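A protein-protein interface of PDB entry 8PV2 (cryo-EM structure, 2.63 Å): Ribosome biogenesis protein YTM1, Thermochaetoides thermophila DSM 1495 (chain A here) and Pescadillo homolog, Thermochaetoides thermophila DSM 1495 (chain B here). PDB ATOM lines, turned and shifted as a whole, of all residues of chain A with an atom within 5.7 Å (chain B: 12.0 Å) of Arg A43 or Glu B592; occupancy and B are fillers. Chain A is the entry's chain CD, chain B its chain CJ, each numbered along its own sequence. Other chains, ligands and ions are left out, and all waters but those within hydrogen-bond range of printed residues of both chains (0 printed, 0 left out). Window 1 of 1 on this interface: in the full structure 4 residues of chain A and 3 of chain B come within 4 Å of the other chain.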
ATOM      1  N   ILE A  41      21.236  -4.457   6.876  1.00  0.00           N
ATOM      2  CA  ILE A  41      21.945  -5.212   5.854  1.00  0.00           C
ATOM      3  C   ILE A  41      21.039  -5.408   4.632  1.00  0.00           C
ATOM      4  O   ILE A  41      19.813  -5.253   4.691  1.00  0.00           O
ATOM      5  CB  ILE A  41      22.439  -6.558   6.414  1.00  0.00           C
ATOM      6  CG1 ILE A  41      23.686  -7.048   5.671  1.00  0.00           C
ATOM      7  CG2 ILE A  41      21.352  -7.614   6.326  1.00  0.00           C
ATOM      8  CD1 ILE A  41      24.401  -8.187   6.363  1.00  0.00           C
ATOM      9  N   ARG A  42      21.668  -5.735   3.506  1.00  0.00           N
ATOM     10  CA  ARG A  42      20.983  -5.956   2.240  1.00  0.00           C
ATOM     11  C   ARG A  42      20.943  -7.462   1.998  1.00  0.00           C
ATOM     12  O   ARG A  42      21.635  -8.216   2.696  1.00  0.00           O
ATOM     13  CB  ARG A  42      21.722  -5.181   1.134  1.00  0.00           C
ATOM     14  CG  ARG A  42      21.177  -5.253  -0.291  1.00  0.00           C
ATOM     15  CD  ARG A  42      19.737  -4.783  -0.354  1.00  0.00           C
ATOM     16  NE  ARG A  42      19.592  -3.423   0.149  1.00  0.00           N
ATOM     17  CZ  ARG A  42      18.427  -2.826   0.363  1.00  0.00           C
ATOM     18  NH1 ARG A  42      17.281  -3.438   0.114  1.00  0.00           N
ATOM     19  NH2 ARG A  42      18.413  -1.583   0.835  1.00  0.00           N
ATOM     20  N   ARG A  43      20.123  -7.926   1.047  1.00  0.00           N
ATOM     21  CA  ARG A  43      20.173  -9.332   0.656  1.00  0.00           C
ATOM     22  C   ARG A  43      21.537  -9.698   0.080  1.00  0.00           C
ATOM     23  O   ARG A  43      21.956 -10.854   0.162  1.00  0.00           O
ATOM     24  CB  ARG A  43      19.070  -9.659  -0.351  1.00  0.00           C
ATOM     25  CG  ARG A  43      19.176  -8.921  -1.672  1.00  0.00           C
ATOM     26  CD  ARG A  43      18.097  -9.374  -2.634  1.00  0.00           C
ATOM     27  NE  ARG A  43      18.319 -10.754  -3.048  1.00  0.00           N
ATOM     28  CZ  ARG A  43      19.117 -11.119  -4.043  1.00  0.00           C
ATOM     29  NH1 ARG A  43      19.782 -10.228  -4.758  1.00  0.00           N
ATOM     30  NH2 ARG A  43      19.253 -12.412  -4.323  1.00  0.00           N
ATOM     31  N   TYR A  44      22.247  -8.723  -0.500  1.00  0.00           N
ATOM     32  CA  TYR A  44      23.634  -8.935  -0.899  1.00  0.00           C
ATOM     33  C   TYR A  44      24.505  -9.241   0.315  1.00  0.00           C
ATOM     34  O   TYR A  44      25.354 -10.140   0.281  1.00  0.00           O
ATOM     35  CB  TYR A  44      24.146  -7.707  -1.663  1.00  0.00           C
ATOM     36  CG  TYR A  44      25.643  -7.670  -1.914  1.00  0.00           C
ATOM     37  CD1 TYR A  44      26.506  -7.016  -1.036  1.00  0.00           C
ATOM     38  CD2 TYR A  44      26.193  -8.295  -3.026  1.00  0.00           C
ATOM     39  CE1 TYR A  44      27.868  -6.985  -1.263  1.00  0.00           C
ATOM     40  CE2 TYR A  44      27.557  -8.268  -3.260  1.00  0.00           C
ATOM     41  CZ  TYR A  44      28.389  -7.610  -2.375  1.00  0.00           C
ATOM     42  OH  TYR A  44      29.745  -7.580  -2.601  1.00  0.00           O
ATOM     43  N   GLY A  45      24.298  -8.498   1.405  1.00  0.00           N
ATOM     44  CA  GLY A  45      25.033  -8.774   2.629  1.00  0.00           C
ATOM     45  C   GLY A  45      24.697 -10.131   3.217  1.00  0.00           C
ATOM     46  O   GLY A  45      25.585 -10.854   3.676  1.00  0.00           O
ATOM     47  N   LEU A  46      23.414 -10.503   3.195  1.00  0.00           N
ATOM     48  CA  LEU A  46      23.014 -11.814   3.696  1.00  0.00           C
ATOM     49  C   LEU A  46      23.562 -12.946   2.829  1.00  0.00           C
ATOM     50  O   LEU A  46      23.953 -13.998   3.353  1.00  0.00           O
ATOM     51  CB  LEU A  46      21.491 -11.893   3.785  1.00  0.00           C
ATOM     52  CG  LEU A  46      20.847 -11.248   5.014  1.00  0.00           C
ATOM     53  CD1 LEU A  46      19.333 -11.235   4.886  1.00  0.00           C
ATOM     54  CD2 LEU A  46      21.271 -11.967   6.285  1.00  0.00           C
ATOM     55  N   SER A  47      23.603 -12.750   1.511  1.00  0.00           N
ATOM     56  CA  SER A  47      24.237 -13.700   0.611  1.00  0.00           C
ATOM     57  C   SER A  47      25.729 -13.833   0.862  1.00  0.00           C
ATOM     58  O   SER A  47      26.245 -14.953   0.833  1.00  0.00           O
ATOM     59  CB  SER A  47      24.003 -13.294  -0.848  1.00  0.00           C
ATOM     60  OG  SER A  47      24.667 -12.081  -1.154  1.00  0.00           O
ATOM     61  N   ARG A  48      26.429 -12.728   1.130  1.00  0.00           N
ATOM     62  CA  ARG A  48      27.835 -12.831   1.508  1.00  0.00           C
ATOM     63  C   ARG A  48      28.017 -13.516   2.858  1.00  0.00           C
ATOM     64  O   ARG A  48      29.031 -14.187   3.073  1.00  0.00           O
ATOM     65  CB  ARG A  48      28.489 -11.449   1.531  1.00  0.00           C
ATOM     66  CG  ARG A  48      28.553 -10.774   0.174  1.00  0.00           C
ATOM     67  CD  ARG A  48      29.223 -11.678  -0.847  1.00  0.00           C
ATOM     68  NE  ARG A  48      30.581 -12.038  -0.458  1.00  0.00           N
ATOM     69  CZ  ARG A  48      31.232 -13.099  -0.916  1.00  0.00           C
ATOM     70  NH1 ARG A  48      30.670 -13.938  -1.771  1.00  0.00           N
ATOM     71  NH2 ARG A  48      32.474 -13.327  -0.501  1.00  0.00           N
ATOM     72  N   PRO A  62      24.539 -17.075  -5.309  1.00  0.00           N
ATOM     73  CA  PRO A  62      23.602 -16.052  -4.817  1.00  0.00           C
ATOM     74  C   PRO A  62      22.336 -16.676  -4.243  1.00  0.00           C
ATOM     75  O   PRO A  62      21.722 -17.553  -4.856  1.00  0.00           O
ATOM     76  CB  PRO A  62      23.294 -15.217  -6.068  1.00  0.00           C
ATOM     77  CG  PRO A  62      23.925 -15.955  -7.239  1.00  0.00           C
ATOM     78  CD  PRO A  62      24.412 -17.283  -6.758  1.00  0.00           C
ATOM     79  N   PHE A  63      21.943 -16.212  -3.060  1.00  0.00           N
ATOM     80  CA  PHE A  63      20.721 -16.652  -2.401  1.00  0.00           C
ATOM     81  C   PHE A  63      19.711 -15.517  -2.284  1.00  0.00           C
ATOM     82  O   PHE A  63      20.070 -14.342  -2.166  1.00  0.00           O
ATOM     83  CB  PHE A  63      21.008 -17.226  -1.008  1.00  0.00           C
ATOM     84  CG  PHE A  63      21.751 -18.540  -1.014  1.00  0.00           C
ATOM     85  CD1 PHE A  63      21.856 -19.302  -2.164  1.00  0.00           C
ATOM     86  CD2 PHE A  63      22.356 -19.003   0.139  1.00  0.00           C
ATOM     87  CE1 PHE A  63      22.534 -20.513  -2.153  1.00  0.00           C
ATOM     88  CE2 PHE A  63      23.039 -20.207   0.155  1.00  0.00           C
ATOM     89  CZ  PHE A  63      23.131 -20.962  -0.991  1.00  0.00           C
ATOM     90  N   ASP A  64      18.437 -15.895  -2.332  1.00  0.00           N
ATOM     91  CA  ASP A  64      17.309 -14.998  -2.161  1.00  0.00           C
ATOM     92  C   ASP A  64      16.430 -15.538  -1.038  1.00  0.00           C
ATOM     93  O   ASP A  64      16.219 -16.749  -0.915  1.00  0.00           O
ATOM     94  CB  ASP A  64      16.524 -14.852  -3.472  1.00  0.00           C
ATOM     95  CG  ASP A  64      15.893 -13.485  -3.627  1.00  0.00           C
ATOM     96  OD1 ASP A  64      16.479 -12.504  -3.125  1.00  0.00           O
ATOM     97  OD2 ASP A  64      14.844 -13.380  -4.297  1.00  0.00           O
ATOM     98  N   PHE A  65      15.933 -14.626  -0.204  1.00  0.00           N
ATOM     99  CA  PHE A  65      15.388 -14.976   1.103  1.00  0.00           C
ATOM    100  C   PHE A  65      13.892 -14.715   1.149  1.00  0.00           C
ATOM    101  O   PHE A  65      13.446 -13.596   0.882  1.00  0.00           O
ATOM    102  CB  PHE A  65      16.088 -14.185   2.216  1.00  0.00           C
ATOM    103  CG  PHE A  65      17.546 -14.511   2.367  1.00  0.00           C
ATOM    104  CD1 PHE A  65      18.496 -13.915   1.553  1.00  0.00           C
ATOM    105  CD2 PHE A  65      17.966 -15.410   3.331  1.00  0.00           C
ATOM    106  CE1 PHE A  65      19.835 -14.221   1.689  1.00  0.00           C
ATOM    107  CE2 PHE A  65      19.306 -15.715   3.477  1.00  0.00           C
ATOM    108  CZ  PHE A  65      20.242 -15.119   2.655  1.00  0.00           C
ATOM    109  N   LEU A  72      12.694 -10.675   0.189  1.00  0.00           N
ATOM    110  CA  LEU A  72      13.327  -9.532   0.841  1.00  0.00           C
ATOM    111  C   LEU A  72      13.796  -8.559  -0.235  1.00  0.00           C
ATOM    112  O   LEU A  72      14.928  -8.652  -0.719  1.00  0.00           O
ATOM    113  CB  LEU A  72      14.488 -10.003   1.709  1.00  0.00           C
ATOM    114  CG  LEU A  72      15.185  -8.978   2.602  1.00  0.00           C
ATOM    115  CD1 LEU A  72      14.372  -8.701   3.856  1.00  0.00           C
ATOM    116  CD2 LEU A  72      16.586  -9.449   2.952  1.00  0.00           C
ATOM    117  N   ARG A  73      12.929  -7.617  -0.607  1.00  0.00           N
ATOM    118  CA  ARG A  73      13.298  -6.576  -1.557  1.00  0.00           C
ATOM    119  C   ARG A  73      13.899  -5.348  -0.892  1.00  0.00           C
ATOM    120  O   ARG A  73      14.703  -4.651  -1.522  1.00  0.00           O
ATOM    121  CB  ARG A  73      12.081  -6.143  -2.385  1.00  0.00           C
ATOM    122  CG  ARG A  73      11.848  -6.937  -3.664  1.00  0.00           C
ATOM    123  CD  ARG A  73      11.022  -8.186  -3.411  1.00  0.00           C
ATOM    124  NE  ARG A  73      10.474  -8.737  -4.645  1.00  0.00           N
ATOM    125  CZ  ARG A  73      11.081  -9.640  -5.403  1.00  0.00           C
ATOM    126  NH1 ARG A  73      12.273 -10.119  -5.088  1.00  0.00           N
ATOM    127  NH2 ARG A  73      10.474 -10.075  -6.504  1.00  0.00           N
ATOM    128  N   SER A  98      19.149 -18.029  -6.118  1.00  0.00           N
ATOM    129  CA  SER A  98      18.555 -16.965  -6.914  1.00  0.00           C
ATOM    130  C   SER A  98      18.549 -17.327  -8.393  1.00  0.00           C
ATOM    131  O   SER A  98      19.317 -18.177  -8.853  1.00  0.00           O
ATOM    132  CB  SER A  98      19.320 -15.658  -6.711  1.00  0.00           C
ATOM    133  OG  SER A  98      19.219 -15.206  -5.373  1.00  0.00           O
ATOM    134  N   PRO A 101      21.017 -14.248 -13.638  1.00  0.00           N
ATOM    135  CA  PRO A 101      20.734 -13.197 -14.615  1.00  0.00           C
ATOM    136  C   PRO A 101      21.597 -13.356 -15.852  1.00  0.00           C
ATOM    137  O   PRO A 101      22.834 -13.316 -15.769  1.00  0.00           O
ATOM    138  CB  PRO A 101      21.074 -11.907 -13.854  1.00  0.00           C
ATOM    139  CG  PRO A 101      22.027 -12.318 -12.773  1.00  0.00           C
ATOM    140  CD  PRO A 101      21.971 -13.814 -12.604  1.00  0.00           C
ATOM    141  N   GLU B 582      11.364   1.107  -7.962  1.00  0.00           N
ATOM    142  CA  GLU B 582      11.626   0.044  -8.925  1.00  0.00           C
ATOM    143  C   GLU B 582      12.999   0.213  -9.565  1.00  0.00           C
ATOM    144  O   GLU B 582      13.731  -0.761  -9.748  1.00  0.00           O
ATOM    145  CB  GLU B 582      10.540   0.019 -10.003  1.00  0.00           C
ATOM    146  N   ALA B 583      13.332   1.460  -9.913  1.00  0.00           N
ATOM    147  CA  ALA B 583      14.637   1.749 -10.501  1.00  0.00           C
ATOM    148  C   ALA B 583      15.763   1.489  -9.509  1.00  0.00           C
ATOM    149  O   ALA B 583      16.809   0.941  -9.880  1.00  0.00           O
ATOM    150  CB  ALA B 583      14.680   3.194 -10.998  1.00  0.00           C
ATOM    151  N   THR B 584      15.567   1.873  -8.245  1.00  0.00           N
ATOM    152  CA  THR B 584      16.561   1.590  -7.214  1.00  0.00           C
ATOM    153  C   THR B 584      16.709   0.094  -6.971  1.00  0.00           C
ATOM    154  O   THR B 584      17.828  -0.390  -6.759  1.00  0.00           O
ATOM    155  CB  THR B 584      16.191   2.301  -5.912  1.00  0.00           C
ATOM    156  N   LEU B 585      15.600  -0.651  -7.001  1.00  0.00           N
ATOM    157  CA  LEU B 585      15.669  -2.102  -6.867  1.00  0.00           C
ATOM    158  C   LEU B 585      16.410  -2.742  -8.034  1.00  0.00           C
ATOM    159  O   LEU B 585      17.211  -3.661  -7.825  1.00  0.00           O
ATOM    160  CB  LEU B 585      14.262  -2.686  -6.750  1.00  0.00           C
ATOM    161  N   GLU B 586      16.163  -2.269  -9.259  1.00  0.00           N
ATOM    162  CA  GLU B 586      16.882  -2.788 -10.420  1.00  0.00           C
ATOM    163  C   GLU B 586      18.369  -2.459 -10.344  1.00  0.00           C
ATOM    164  O   GLU B 586      19.213  -3.288 -10.710  1.00  0.00           O
ATOM    165  CB  GLU B 586      16.273  -2.229 -11.705  1.00  0.00           C
ATOM    166  N   ARG B 587      18.706  -1.257  -9.869  1.00  0.00           N
ATOM    167  CA  ARG B 587      20.108  -0.895  -9.675  1.00  0.00           C
ATOM    168  C   ARG B 587      20.773  -1.763  -8.614  1.00  0.00           C
ATOM    169  O   ARG B 587      21.930  -2.158  -8.780  1.00  0.00           O
ATOM    170  CB  ARG B 587      20.223   0.582  -9.300  1.00  0.00           C
ATOM    171  N   GLN B 588      20.058  -2.071  -7.528  1.00  0.00           N
ATOM    172  CA  GLN B 588      20.599  -2.960  -6.502  1.00  0.00           C
ATOM    173  C   GLN B 588      20.801  -4.374  -7.038  1.00  0.00           C
ATOM    174  O   GLN B 588      21.801  -5.028  -6.712  1.00  0.00           O
ATOM    175  CB  GLN B 588      19.677  -2.975  -5.284  1.00  0.00           C
ATOM    176  N   ARG B 589      19.859  -4.862  -7.852  1.00  0.00           N
ATOM    177  CA  ARG B 589      20.018  -6.174  -8.474  1.00  0.00           C
ATOM    178  C   ARG B 589      21.210  -6.208  -9.422  1.00  0.00           C
ATOM    179  O   ARG B 589      21.964  -7.187  -9.430  1.00  0.00           O
ATOM    180  CB  ARG B 589      18.745  -6.572  -9.220  1.00  0.00           C
ATOM    181  CG  ARG B 589      17.547  -6.832  -8.325  1.00  0.00           C
ATOM    182  CD  ARG B 589      17.745  -8.062  -7.461  1.00  0.00           C
ATOM    183  NE  ARG B 589      16.577  -8.325  -6.631  1.00  0.00           N
ATOM    184  CZ  ARG B 589      16.389  -7.809  -5.424  1.00  0.00           C
ATOM    185  NH1 ARG B 589      17.267  -6.980  -4.883  1.00  0.00           N
ATOM    186  NH2 ARG B 589      15.289  -8.126  -4.747  1.00  0.00           N
ATOM    187  N   GLU B 590      21.399  -5.149 -10.214  1.00  0.00           N
ATOM    188  CA  GLU B 590      22.563  -5.074 -11.092  1.00  0.00           C
ATOM    189  C   GLU B 590      23.858  -5.008 -10.290  1.00  0.00           C
ATOM    190  O   GLU B 590      24.863  -5.618 -10.674  1.00  0.00           O
ATOM    191  CB  GLU B 590      22.442  -3.866 -12.019  1.00  0.00           C
ATOM    192  N   LEU B 591      23.848  -4.274  -9.173  1.00  0.00           N
ATOM    193  CA  LEU B 591      25.033  -4.172  -8.329  1.00  0.00           C
ATOM    194  C   LEU B 591      25.396  -5.505  -7.687  1.00  0.00           C
ATOM    195  O   LEU B 591      26.580  -5.852  -7.620  1.00  0.00           O
ATOM    196  CB  LEU B 591      24.819  -3.108  -7.253  1.00  0.00           C
ATOM    197  N   GLU B 592      24.404  -6.266  -7.210  1.00  0.00           N
ATOM    198  CA  GLU B 592      24.728  -7.553  -6.604  1.00  0.00           C
ATOM    199  C   GLU B 592      25.086  -8.594  -7.659  1.00  0.00           C
ATOM    200  O   GLU B 592      25.884  -9.498  -7.386  1.00  0.00           O
ATOM    201  CB  GLU B 592      23.580  -8.050  -5.717  1.00  0.00           C
ATOM    202  CG  GLU B 592      22.243  -8.272  -6.408  1.00  0.00           C
ATOM    203  CD  GLU B 592      22.091  -9.675  -6.972  1.00  0.00           C
ATOM    204  OE1 GLU B 592      22.866 -10.567  -6.571  1.00  0.00           O
ATOM    205  OE2 GLU B 592      21.200  -9.883  -7.824  1.00  0.00           O
ATOM    206  N   ALA B 593      24.516  -8.489  -8.863  1.00  0.00           N
ATOM    207  CA  ALA B 593      24.897  -9.403  -9.932  1.00  0.00           C
ATOM    208  C   ALA B 593      26.273  -9.082 -10.497  1.00  0.00           C
ATOM    209  O   ALA B 593      26.927  -9.977 -11.043  1.00  0.00           O
ATOM    210  CB  ALA B 593      23.852  -9.375 -11.048  1.00  0.00           C
ATOM    211  N   GLU B 594      26.723  -7.838 -10.379  1.00  0.00           N
ATOM    212  CA  GLU B 594      28.050  -7.458 -10.844  1.00  0.00           C
ATOM    213  C   GLU B 594      29.131  -7.993  -9.907  1.00  0.00           C
ATOM    214  O   GLU B 594      28.840  -8.450  -8.802  1.00  0.00           O
ATOM    215  CB  GLU B 594      28.162  -5.938 -10.964  1.00  0.00           C
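OE2 of Glu B592 lies within salt-bridge range of NH1 of Arg A43 (3.4 Å).
The backbone carbonyl oxygen (O) of Arg A73 lies within hydrogen-bond range of the guanidinium group (NH1) of Arg A42 (3.3 Å). The side-chain hydroxyl of Ser A47 is in hydrogen-bond range of the backbone carbonyl oxygen of Arg A43, 3.3 Å away. The guanidinium group of Arg A43 lies within hydrogen-bond range of the backbone carbonyl oxygen of Phe A63. The guanidinium group (NE) of Arg A43 is in salt-bridge range of the side-chain carboxylate (OD1) of Asp A64 (2.5 Å). The guanidinium group (NH2) of Arg A43 is in hydrogen-bond range of the side-chain hydroxyl (OG) of Ser A98 (3.0 Å). O of Tyr A44 lies within hydrogen-bond range of OG of Ser A47.
Among the printed residues, pairs that only touch across the chains: Arg A43 with Arg B589 (3.4 Å), Tyr A44 with Glu B592 (3.8 Å), Arg A73 with Arg B589 (3.6 Å) and Pro A101 with Ala B593 (3.9 Å).
No residue of chain B comes within 4 Å of Ile A41. Of the printed residues of chain B, Arg A43 touches Arg B589 and Glu B592. Tyr A44 touches just one residue of chain B: Glu B592 (3.8 Å). No residue of chain B comes within 4 Å of Gly A45. Ser A47 touches none of the printed residues of chain B. Pro A62 touches none of the printed residues of chain B. Asp A64 touches none of the printed residues of chain B. No residue of chain B comes within 4 Å of Phe A65. No residue of chain B comes within 4 Å of Leu A72. Printed residues of chain B within 4 Å of Arg A73: Arg B589. Printed residues of chain B within 4 Å of Pro A101: Ala B593 (3.9 Å). Printed residues of chain A within 4 Å of Arg B589: Arg A43 and Arg A73. Glu B592 touches just these residues of chain A: Arg A43 and Tyr A44. Printed residues of chain A within 4 Å of Ala B593: Pro A101 (3.9 Å).
Of the 13 printed residues of chain B, 3 touch a printed residue of chain A. Of the 16 printed residues of chain A, 4 touch a printed residue of chain B. Printed residues of chain A that touch a printed residue of chain B: Arg A43, Tyr A44, Arg A73 and Pro A101. Among the printed residues, 5 pairs touch across the chains. Among the printed residues, Asp or Glu carboxylates within 4 Å of a Lys or Arg side-chain nitrogen of the other chain: Arg A43 with Glu B592.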
